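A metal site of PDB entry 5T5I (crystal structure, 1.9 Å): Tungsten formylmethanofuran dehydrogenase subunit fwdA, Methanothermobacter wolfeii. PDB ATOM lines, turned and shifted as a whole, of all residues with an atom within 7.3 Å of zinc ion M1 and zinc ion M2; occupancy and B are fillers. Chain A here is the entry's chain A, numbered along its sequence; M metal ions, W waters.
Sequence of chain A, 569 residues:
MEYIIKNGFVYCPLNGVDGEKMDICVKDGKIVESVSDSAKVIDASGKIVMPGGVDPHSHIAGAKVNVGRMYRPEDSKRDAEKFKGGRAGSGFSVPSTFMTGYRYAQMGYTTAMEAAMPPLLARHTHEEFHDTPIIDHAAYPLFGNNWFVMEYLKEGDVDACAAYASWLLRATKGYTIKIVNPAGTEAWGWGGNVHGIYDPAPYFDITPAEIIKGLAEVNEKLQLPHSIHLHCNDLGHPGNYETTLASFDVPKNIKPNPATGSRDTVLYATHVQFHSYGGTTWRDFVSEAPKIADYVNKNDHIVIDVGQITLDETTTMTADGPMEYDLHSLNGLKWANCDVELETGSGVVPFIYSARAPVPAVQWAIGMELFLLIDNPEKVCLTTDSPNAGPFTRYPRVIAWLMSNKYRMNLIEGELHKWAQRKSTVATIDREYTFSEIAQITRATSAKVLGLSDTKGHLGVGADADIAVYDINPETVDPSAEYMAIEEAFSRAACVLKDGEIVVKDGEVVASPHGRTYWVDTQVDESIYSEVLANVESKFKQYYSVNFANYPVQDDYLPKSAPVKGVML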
ATOM      1  N   HIS A  57      22.355 -22.692 -15.855  1.00  0.00           N
ATOM      2  CA  HIS A  57      22.446 -21.517 -16.721  1.00  0.00           C
ATOM      3  C   HIS A  57      23.876 -21.010 -16.855  1.00  0.00           C
ATOM      4  O   HIS A  57      24.364 -20.293 -15.986  1.00  0.00           O
ATOM      5  CB  HIS A  57      21.535 -20.397 -16.154  1.00  0.00           C
ATOM      6  CG  HIS A  57      21.337 -19.265 -17.119  1.00  0.00           C
ATOM      7  ND1 HIS A  57      20.121 -19.086 -17.746  1.00  0.00           N
ATOM      8  CD2 HIS A  57      22.204 -18.336 -17.566  1.00  0.00           C
ATOM      9  CE1 HIS A  57      20.265 -18.032 -18.510  1.00  0.00           C
ATOM     10  NE2 HIS A  57      21.512 -17.543 -18.461  1.00  0.00           N
ATOM     11  N   SER A  58      24.534 -21.341 -17.972  1.00  0.00           N
ATOM     12  CA  SER A  58      25.890 -20.886 -18.251  1.00  0.00           C
ATOM     13  C   SER A  58      26.071 -20.652 -19.760  1.00  0.00           C
ATOM     14  O   SER A  58      25.350 -21.266 -20.562  1.00  0.00           O
ATOM     15  CB  SER A  58      26.909 -21.909 -17.750  1.00  0.00           C
ATOM     16  OG  SER A  58      28.183 -21.319 -17.587  1.00  0.00           O
ATOM     17  N   HIS A  59      26.968 -19.745 -20.130  1.00  0.00           N
ATOM     18  CA  HIS A  59      27.286 -19.440 -21.543  1.00  0.00           C
ATOM     19  C   HIS A  59      28.640 -20.073 -21.797  1.00  0.00           C
ATOM     20  O   HIS A  59      29.698 -19.499 -21.431  1.00  0.00           O
ATOM     21  CB  HIS A  59      27.252 -17.925 -21.807  1.00  0.00           C
ATOM     22  CG  HIS A  59      25.872 -17.379 -21.608  1.00  0.00           C
ATOM     23  ND1 HIS A  59      24.930 -17.408 -22.616  1.00  0.00           N
ATOM     24  CD2 HIS A  59      25.283 -16.873 -20.493  1.00  0.00           C
ATOM     25  CE1 HIS A  59      23.831 -16.887 -22.119  1.00  0.00           C
ATOM     26  NE2 HIS A  59      23.978 -16.604 -20.820  1.00  0.00           N
ATOM     27  N   ALA A 115      22.973 -21.822 -22.065  1.00  0.00           N
ATOM     28  CA  ALA A 115      21.773 -21.008 -21.826  1.00  0.00           C
ATOM     29  C   ALA A 115      21.147 -20.321 -23.028  1.00  0.00           C
ATOM     30  O   ALA A 115      20.017 -19.873 -22.883  1.00  0.00           O
ATOM     31  CB  ALA A 115      22.088 -19.950 -20.775  1.00  0.00           C
ATOM     32  N   ALA A 116      21.831 -20.150 -24.149  1.00  0.00           N
ATOM     33  CA  ALA A 116      21.260 -19.348 -25.244  1.00  0.00           C
ATOM     34  C   ALA A 116      21.866 -19.729 -26.596  1.00  0.00           C
ATOM     35  O   ALA A 116      22.894 -19.178 -26.991  1.00  0.00           O
ATOM     36  CB  ALA A 116      21.522 -17.867 -24.961  1.00  0.00           C
ATOM     37  N   KCX A 178      13.787 -21.084 -24.320  1.00  0.00           N
ATOM     38  CA  KCX A 178      14.475 -19.930 -23.717  1.00  0.00           C
ATOM     39  CB  KCX A 178      15.976 -20.057 -23.982  1.00  0.00           C
ATOM     40  CG  KCX A 178      16.785 -18.883 -23.425  1.00  0.00           C
ATOM     41  CD  KCX A 178      16.892 -18.909 -21.901  1.00  0.00           C
ATOM     42  CE  KCX A 178      17.446 -17.604 -21.352  1.00  0.00           C
ATOM     43  NZ  KCX A 178      18.847 -17.449 -21.661  1.00  0.00           N
ATOM     44  C   KCX A 178      13.925 -18.655 -24.306  1.00  0.00           C
ATOM     45  O   KCX A 178      13.770 -18.565 -25.530  1.00  0.00           O
ATOM     46  CX  KCX A 178      19.537 -16.426 -21.161  1.00  0.00           C
ATOM     47  OQ1 KCX A 178      20.836 -16.395 -21.377  1.00  0.00           O
ATOM     48  OQ2 KCX A 178      19.040 -15.535 -20.475  1.00  0.00           O
ATOM     49  N   ILE A 179      13.602 -17.676 -23.432  1.00  0.00           N
ATOM     50  CA  ILE A 179      13.019 -16.385 -23.795  1.00  0.00           C
ATOM     51  C   ILE A 179      13.934 -15.281 -23.233  1.00  0.00           C
ATOM     52  O   ILE A 179      14.053 -15.150 -22.008  1.00  0.00           O
ATOM     53  CB  ILE A 179      11.582 -16.259 -23.260  1.00  0.00           C
ATOM     54  CG1 ILE A 179      10.730 -17.528 -23.603  1.00  0.00           C
ATOM     55  CG2 ILE A 179      10.925 -14.982 -23.777  1.00  0.00           C
ATOM     56  CD1 ILE A 179       9.362 -17.585 -22.875  1.00  0.00           C
ATOM     57  N   VAL A 180      14.511 -14.460 -24.129  1.00  0.00           N
ATOM     58  CA  VAL A 180      15.411 -13.339 -23.786  1.00  0.00           C
ATOM     59  C   VAL A 180      14.871 -12.035 -24.345  1.00  0.00           C
ATOM     60  O   VAL A 180      14.829 -11.870 -25.576  1.00  0.00           O
ATOM     61  CB  VAL A 180      16.859 -13.581 -24.305  1.00  0.00           C
ATOM     62  CG1 VAL A 180      17.764 -12.364 -24.032  1.00  0.00           C
ATOM     63  CG2 VAL A 180      17.455 -14.853 -23.711  1.00  0.00           C
ATOM     64  N   ASN A 181      14.518 -11.088 -23.463  1.00  0.00           N
ATOM     65  CA  ASN A 181      14.025  -9.752 -23.861  1.00  0.00           C
ATOM     66  C   ASN A 181      12.957  -9.904 -24.967  1.00  0.00           C
ATOM     67  O   ASN A 181      13.173  -9.480 -26.106  1.00  0.00           O
ATOM     68  CB  ASN A 181      15.181  -8.881 -24.330  1.00  0.00           C
ATOM     69  CG  ASN A 181      14.799  -7.432 -24.598  1.00  0.00           C
ATOM     70  OD1 ASN A 181      13.790  -6.928 -24.117  1.00  0.00           O
ATOM     71  ND2 ASN A 181      15.571  -6.765 -25.429  1.00  0.00           N
ATOM     72  N   HIS A 229      12.076 -20.575 -19.691  1.00  0.00           N
ATOM     73  CA  HIS A 229      13.264 -20.056 -18.982  1.00  0.00           C
ATOM     74  C   HIS A 229      13.413 -18.592 -19.440  1.00  0.00           C
ATOM     75  O   HIS A 229      13.707 -18.353 -20.598  1.00  0.00           O
ATOM     76  CB  HIS A 229      14.433 -20.976 -19.350  1.00  0.00           C
ATOM     77  CG  HIS A 229      15.656 -20.865 -18.499  1.00  0.00           C
ATOM     78  ND1 HIS A 229      16.085 -21.924 -17.713  1.00  0.00           N
ATOM     79  CD2 HIS A 229      16.568 -19.869 -18.404  1.00  0.00           C
ATOM     80  CE1 HIS A 229      17.234 -21.552 -17.185  1.00  0.00           C
ATOM     81  NE2 HIS A 229      17.571 -20.317 -17.553  1.00  0.00           N
ATOM     82  N   LEU A 230      13.045 -17.639 -18.563  1.00  0.00           N
ATOM     83  CA  LEU A 230      12.877 -16.222 -18.906  1.00  0.00           C
ATOM     84  C   LEU A 230      13.908 -15.248 -18.369  1.00  0.00           C
ATOM     85  O   LEU A 230      14.143 -15.176 -17.159  1.00  0.00           O
ATOM     86  CB  LEU A 230      11.480 -15.787 -18.411  1.00  0.00           C
ATOM     87  CG  LEU A 230      11.056 -14.323 -18.648  1.00  0.00           C
ATOM     88  CD1 LEU A 230      10.968 -13.980 -20.153  1.00  0.00           C
ATOM     89  CD2 LEU A 230       9.758 -14.032 -17.939  1.00  0.00           C
ATOM     90  N   HIS A 231      14.470 -14.449 -19.291  1.00  0.00           N
ATOM     91  CA  HIS A 231      15.339 -13.290 -19.063  1.00  0.00           C
ATOM     92  C   HIS A 231      14.401 -12.124 -19.444  1.00  0.00           C
ATOM     93  O   HIS A 231      14.053 -11.945 -20.619  1.00  0.00           O
ATOM     94  CB  HIS A 231      16.616 -13.411 -19.934  1.00  0.00           C
ATOM     95  CG  HIS A 231      17.403 -12.150 -20.259  1.00  0.00           C
ATOM     96  ND1 HIS A 231      18.768 -12.220 -20.472  1.00  0.00           N
ATOM     97  CD2 HIS A 231      16.991 -10.904 -20.599  1.00  0.00           C
ATOM     98  CE1 HIS A 231      19.146 -10.998 -20.820  1.00  0.00           C
ATOM     99  NE2 HIS A 231      18.107 -10.182 -20.918  1.00  0.00           N
ATOM    100  N   CYS A 232      13.923 -11.379 -18.419  1.00  0.00           N
ATOM    101  CA  CYS A 232      12.923 -10.318 -18.577  1.00  0.00           C
ATOM    102  C   CYS A 232      13.337  -9.162 -19.458  1.00  0.00           C
ATOM    103  O   CYS A 232      14.522  -8.879 -19.638  1.00  0.00           O
ATOM    104  CB  CYS A 232      12.462  -9.794 -17.204  1.00  0.00           C
ATOM    105  SG  CYS A 232      11.616 -11.011 -16.160  1.00  0.00           S
ATOM    106  N   LEU A 235      16.235  -5.280 -18.663  1.00  0.00           N
ATOM    107  CA  LEU A 235      17.376  -5.698 -17.853  1.00  0.00           C
ATOM    108  C   LEU A 235      18.298  -4.509 -17.529  1.00  0.00           C
ATOM    109  O   LEU A 235      18.605  -3.700 -18.395  1.00  0.00           O
ATOM    110  CB  LEU A 235      18.214  -6.783 -18.555  1.00  0.00           C
ATOM    111  CG  LEU A 235      19.304  -7.497 -17.694  1.00  0.00           C
ATOM    112  CD1 LEU A 235      19.621  -8.882 -18.231  1.00  0.00           C
ATOM    113  CD2 LEU A 235      20.662  -6.755 -17.676  1.00  0.00           C
ATOM    114  N   THR A 270      15.602 -16.317 -14.720  1.00  0.00           N
ATOM    115  CA  THR A 270      17.069 -16.336 -14.610  1.00  0.00           C
ATOM    116  C   THR A 270      17.665 -14.981 -14.206  1.00  0.00           C
ATOM    117  O   THR A 270      17.125 -13.912 -14.508  1.00  0.00           O
ATOM    118  CB  THR A 270      17.697 -16.920 -15.908  1.00  0.00           C
ATOM    119  OG1 THR A 270      19.099 -17.129 -15.682  1.00  0.00           O
ATOM    120  CG2 THR A 270      17.454 -16.037 -17.147  1.00  0.00           C
ATOM    121  N   HIS A 271      18.844 -15.042 -13.551  1.00  0.00           N
ATOM    122  CA  HIS A 271      19.675 -13.936 -13.095  1.00  0.00           C
ATOM    123  C   HIS A 271      18.855 -12.726 -12.631  1.00  0.00           C
ATOM    124  O   HIS A 271      19.014 -11.605 -13.106  1.00  0.00           O
ATOM    125  CB  HIS A 271      20.728 -13.565 -14.161  1.00  0.00           C
ATOM    126  CG  HIS A 271      20.218 -13.366 -15.562  1.00  0.00           C
ATOM    127  ND1 HIS A 271      19.377 -12.326 -15.900  1.00  0.00           N
ATOM    128  CD2 HIS A 271      20.464 -14.095 -16.678  1.00  0.00           C
ATOM    129  CE1 HIS A 271      19.145 -12.459 -17.203  1.00  0.00           C
ATOM    130  NE2 HIS A 271      19.771 -13.508 -17.703  1.00  0.00           N
ATOM    131  N   PHE A 274      19.783  -8.794 -11.743  1.00  0.00           N
ATOM    132  CA  PHE A 274      19.745  -7.720 -12.753  1.00  0.00           C
ATOM    133  C   PHE A 274      18.326  -7.147 -13.032  1.00  0.00           C
ATOM    134  O   PHE A 274      18.198  -6.198 -13.805  1.00  0.00           O
ATOM    135  CB  PHE A 274      20.332  -8.204 -14.098  1.00  0.00           C
ATOM    136  CG  PHE A 274      21.796  -8.558 -14.119  1.00  0.00           C
ATOM    137  CD1 PHE A 274      22.765  -7.564 -14.185  1.00  0.00           C
ATOM    138  CD2 PHE A 274      22.198  -9.881 -14.199  1.00  0.00           C
ATOM    139  CE1 PHE A 274      24.124  -7.892 -14.290  1.00  0.00           C
ATOM    140  CE2 PHE A 274      23.559 -10.203 -14.326  1.00  0.00           C
ATOM    141  CZ  PHE A 274      24.516  -9.207 -14.351  1.00  0.00           C
ATOM    142  N   HIS A 275      17.283  -7.754 -12.439  1.00  0.00           N
ATOM    143  CA  HIS A 275      15.883  -7.427 -12.597  1.00  0.00           C
ATOM    144  C   HIS A 275      15.234  -6.934 -11.271  1.00  0.00           C
ATOM    145  O   HIS A 275      14.017  -6.802 -11.217  1.00  0.00           O
ATOM    146  CB  HIS A 275      15.187  -8.699 -13.108  1.00  0.00           C
ATOM    147  CG  HIS A 275      15.685  -9.125 -14.445  1.00  0.00           C
ATOM    148  ND1 HIS A 275      15.438  -8.355 -15.576  1.00  0.00           N
ATOM    149  CD2 HIS A 275      16.465 -10.172 -14.789  1.00  0.00           C
ATOM    150  CE1 HIS A 275      16.046  -8.991 -16.575  1.00  0.00           C
ATOM    151  NE2 HIS A 275      16.649 -10.095 -16.149  1.00  0.00           N
ATOM    152  N   MET A 317      27.928 -11.353 -22.233  1.00  0.00           N
ATOM    153  CA  MET A 317      27.527 -11.972 -23.495  1.00  0.00           C
ATOM    154  C   MET A 317      26.102 -12.519 -23.328  1.00  0.00           C
ATOM    155  O   MET A 317      25.853 -13.390 -22.479  1.00  0.00           O
ATOM    156  CB  MET A 317      28.499 -13.079 -23.904  1.00  0.00           C
ATOM    157  CG  MET A 317      28.835 -14.070 -22.795  1.00  0.00           C
ATOM    158  SD  MET A 317      29.894 -15.418 -23.351  1.00  0.00           S
ATOM    159  CE  MET A 317      31.346 -14.492 -23.876  1.00  0.00           C
ATOM    160  N   THR A 318      25.156 -11.960 -24.064  1.00  0.00           N
ATOM    161  CA  THR A 318      23.765 -12.371 -23.946  1.00  0.00           C
ATOM    162  C   THR A 318      23.097 -12.306 -25.299  1.00  0.00           C
ATOM    163  O   THR A 318      23.654 -11.704 -26.220  1.00  0.00           O
ATOM    164  CB  THR A 318      22.994 -11.430 -22.952  1.00  0.00           C
ATOM    165  OG1 THR A 318      22.882 -10.123 -23.516  1.00  0.00           O
ATOM    166  CG2 THR A 318      23.608 -11.375 -21.555  1.00  0.00           C
ATOM    167  N   ALA A 319      21.872 -12.844 -25.398  1.00  0.00           N
ATOM    168  CA  ALA A 319      21.048 -12.696 -26.602  1.00  0.00           C
ATOM    169  C   ALA A 319      20.209 -11.392 -26.488  1.00  0.00           C
ATOM    170  O   ALA A 319      19.212 -11.252 -27.196  1.00  0.00           O
ATOM    171  CB  ALA A 319      20.130 -13.909 -26.783  1.00  0.00           C
ATOM    172  N   ASP A 320      20.587 -10.442 -25.597  1.00  0.00           N
ATOM    173  CA  ASP A 320      19.891  -9.167 -25.395  1.00  0.00           C
ATOM    174  C   ASP A 320      20.750  -8.107 -26.095  1.00  0.00           C
ATOM    175  O   ASP A 320      21.448  -7.335 -25.462  1.00  0.00           O
ATOM    176  CB  ASP A 320      19.726  -8.900 -23.899  1.00  0.00           C
ATOM    177  CG  ASP A 320      18.722  -7.821 -23.527  1.00  0.00           C
ATOM    178  OD1 ASP A 320      18.418  -6.953 -24.407  1.00  0.00           O
ATOM    179  OD2 ASP A 320      18.295  -7.787 -22.364  1.00  0.00           O
ATOM    180  N   MET A 323      20.547  -4.256 -24.946  1.00  0.00           N
ATOM    181  CA  MET A 323      21.156  -4.046 -23.639  1.00  0.00           C
ATOM    182  C   MET A 323      22.701  -3.992 -23.775  1.00  0.00           C
ATOM    183  O   MET A 323      23.350  -3.160 -23.153  1.00  0.00           O
ATOM    184  CB  MET A 323      20.753  -5.165 -22.661  1.00  0.00           C
ATOM    185  CG  MET A 323      21.357  -5.016 -21.272  1.00  0.00           C
ATOM    186  SD  MET A 323      23.038  -5.659 -21.067  1.00  0.00           S
ATOM    187  CE  MET A 323      22.757  -7.412 -21.202  1.00  0.00           C
ATOM    188  N   ASP A 385      25.155 -16.076 -14.074  1.00  0.00           N
ATOM    189  CA  ASP A 385      24.880 -15.922 -15.515  1.00  0.00           C
ATOM    190  C   ASP A 385      26.217 -16.015 -16.266  1.00  0.00           C
ATOM    191  O   ASP A 385      26.517 -15.193 -17.134  1.00  0.00           O
ATOM    192  CB  ASP A 385      24.174 -14.594 -15.828  1.00  0.00           C
ATOM    193  CG  ASP A 385      23.696 -14.480 -17.282  1.00  0.00           C
ATOM    194  OD1 ASP A 385      23.522 -15.539 -17.930  1.00  0.00           O
ATOM    195  OD2 ASP A 385      23.477 -13.343 -17.758  1.00  0.00           O
ATOM    196  N   SER A 386      27.059 -16.971 -15.858  1.00  0.00           N
ATOM    197  CA  SER A 386      28.451 -17.051 -16.291  1.00  0.00           C
ATOM    198  C   SER A 386      28.654 -16.828 -17.763  1.00  0.00           C
ATOM    199  O   SER A 386      27.956 -17.460 -18.558  1.00  0.00           O
ATOM    200  CB  SER A 386      29.096 -18.366 -15.871  1.00  0.00           C
ATOM    201  OG  SER A 386      30.482 -18.360 -16.169  1.00  0.00           O
ATOM    202  N   ASN A 388      28.636 -13.353 -17.353  1.00  0.00           N
ATOM    203  CA  ASN A 388      28.038 -12.016 -17.213  1.00  0.00           C
ATOM    204  C   ASN A 388      28.168 -11.343 -15.850  1.00  0.00           C
ATOM    205  O   ASN A 388      28.538 -10.166 -15.822  1.00  0.00           O
ATOM    206  CB  ASN A 388      26.586 -12.013 -17.621  1.00  0.00           C
ATOM    207  CG  ASN A 388      26.387 -12.171 -19.082  1.00  0.00           C
ATOM    208  OD1 ASN A 388      26.425 -11.190 -19.814  1.00  0.00           O
ATOM    209  ND2 ASN A 388      26.146 -13.392 -19.535  1.00  0.00           N
HETATM  210 ZN    ZN M   1      19.992 -13.852 -19.828  1.00  0.00          ZN
HETATM  211 ZN    ZN M   2      22.343 -16.000 -19.658  1.00  0.00          ZN
HETATM  212  O   HOH W   1      21.352 -14.228 -22.846  1.00  0.00           O
HETATM  213  O   HOH W   2      21.954 -14.041 -19.916  1.00  0.00           O
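Of the 26 residues printed, 3 come within 4 Å of zinc ion M1.
The nearest printed residue that does not touch zinc ion M1 is Asp 385 (4.1 Å).
Zinc ion M2 is bound by water W2.
Zinc ion M2 is bound by NE2 of His 59 (2.1 Å).
Zinc ion M2 is bound by NE2 of His 57 (2.1 Å).
OD1 of Asp 385 is bound to zinc ion M2 (2.1 Å).
Zinc ion M2 is bound by OQ1 of KCX 178 (2.3 Å).
Zinc ion M2 has five donor atoms within binding distance.
The backbone NH (N) of His 59 sits at hydrogen-bond distance from the backbone carbonyl oxygen (O) of Ser 386 (2.9 Å).
The backbone carbonyl oxygen of His 231 lies within hydrogen-bond range of the backbone NH of Asn 181, at 3.0 Å.
A ring nitrogen (NE2) of His 229 sits at hydrogen-bond distance from a ring nitrogen (ND1) of His 57 (2.8 Å).
OG1 of Thr 270 sits at hydrogen-bond distance from ND1 of His 57, at 3.0 Å.
The side-chain amide nitrogen of Asn 388 is in hydrogen-bond range of the backbone carbonyl oxygen of Asp 385 (3.0 Å).
The backbone carbonyl oxygen (O) of Ala 115 is in hydrogen-bond range of NZ of KCX 178 (3.0 Å).
A ring nitrogen (NE2) of His 231 sits at hydrogen-bond distance from the side-chain carboxylate of Asp 320, 2.8 Å away.
N of His 231 is in hydrogen-bond range of O of Ile 179 (2.8 Å).
Zinc ion M1 is bound by water W2 (2.0 Å), OQ2 of KCX 178 (2.0 Å), a ring nitrogen (ND1) of His 231 (2.1 Å) and a ring nitrogen (NE2) of His 271 (2.2 Å).
Zinc ion M1 has four donor atoms within binding distance.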
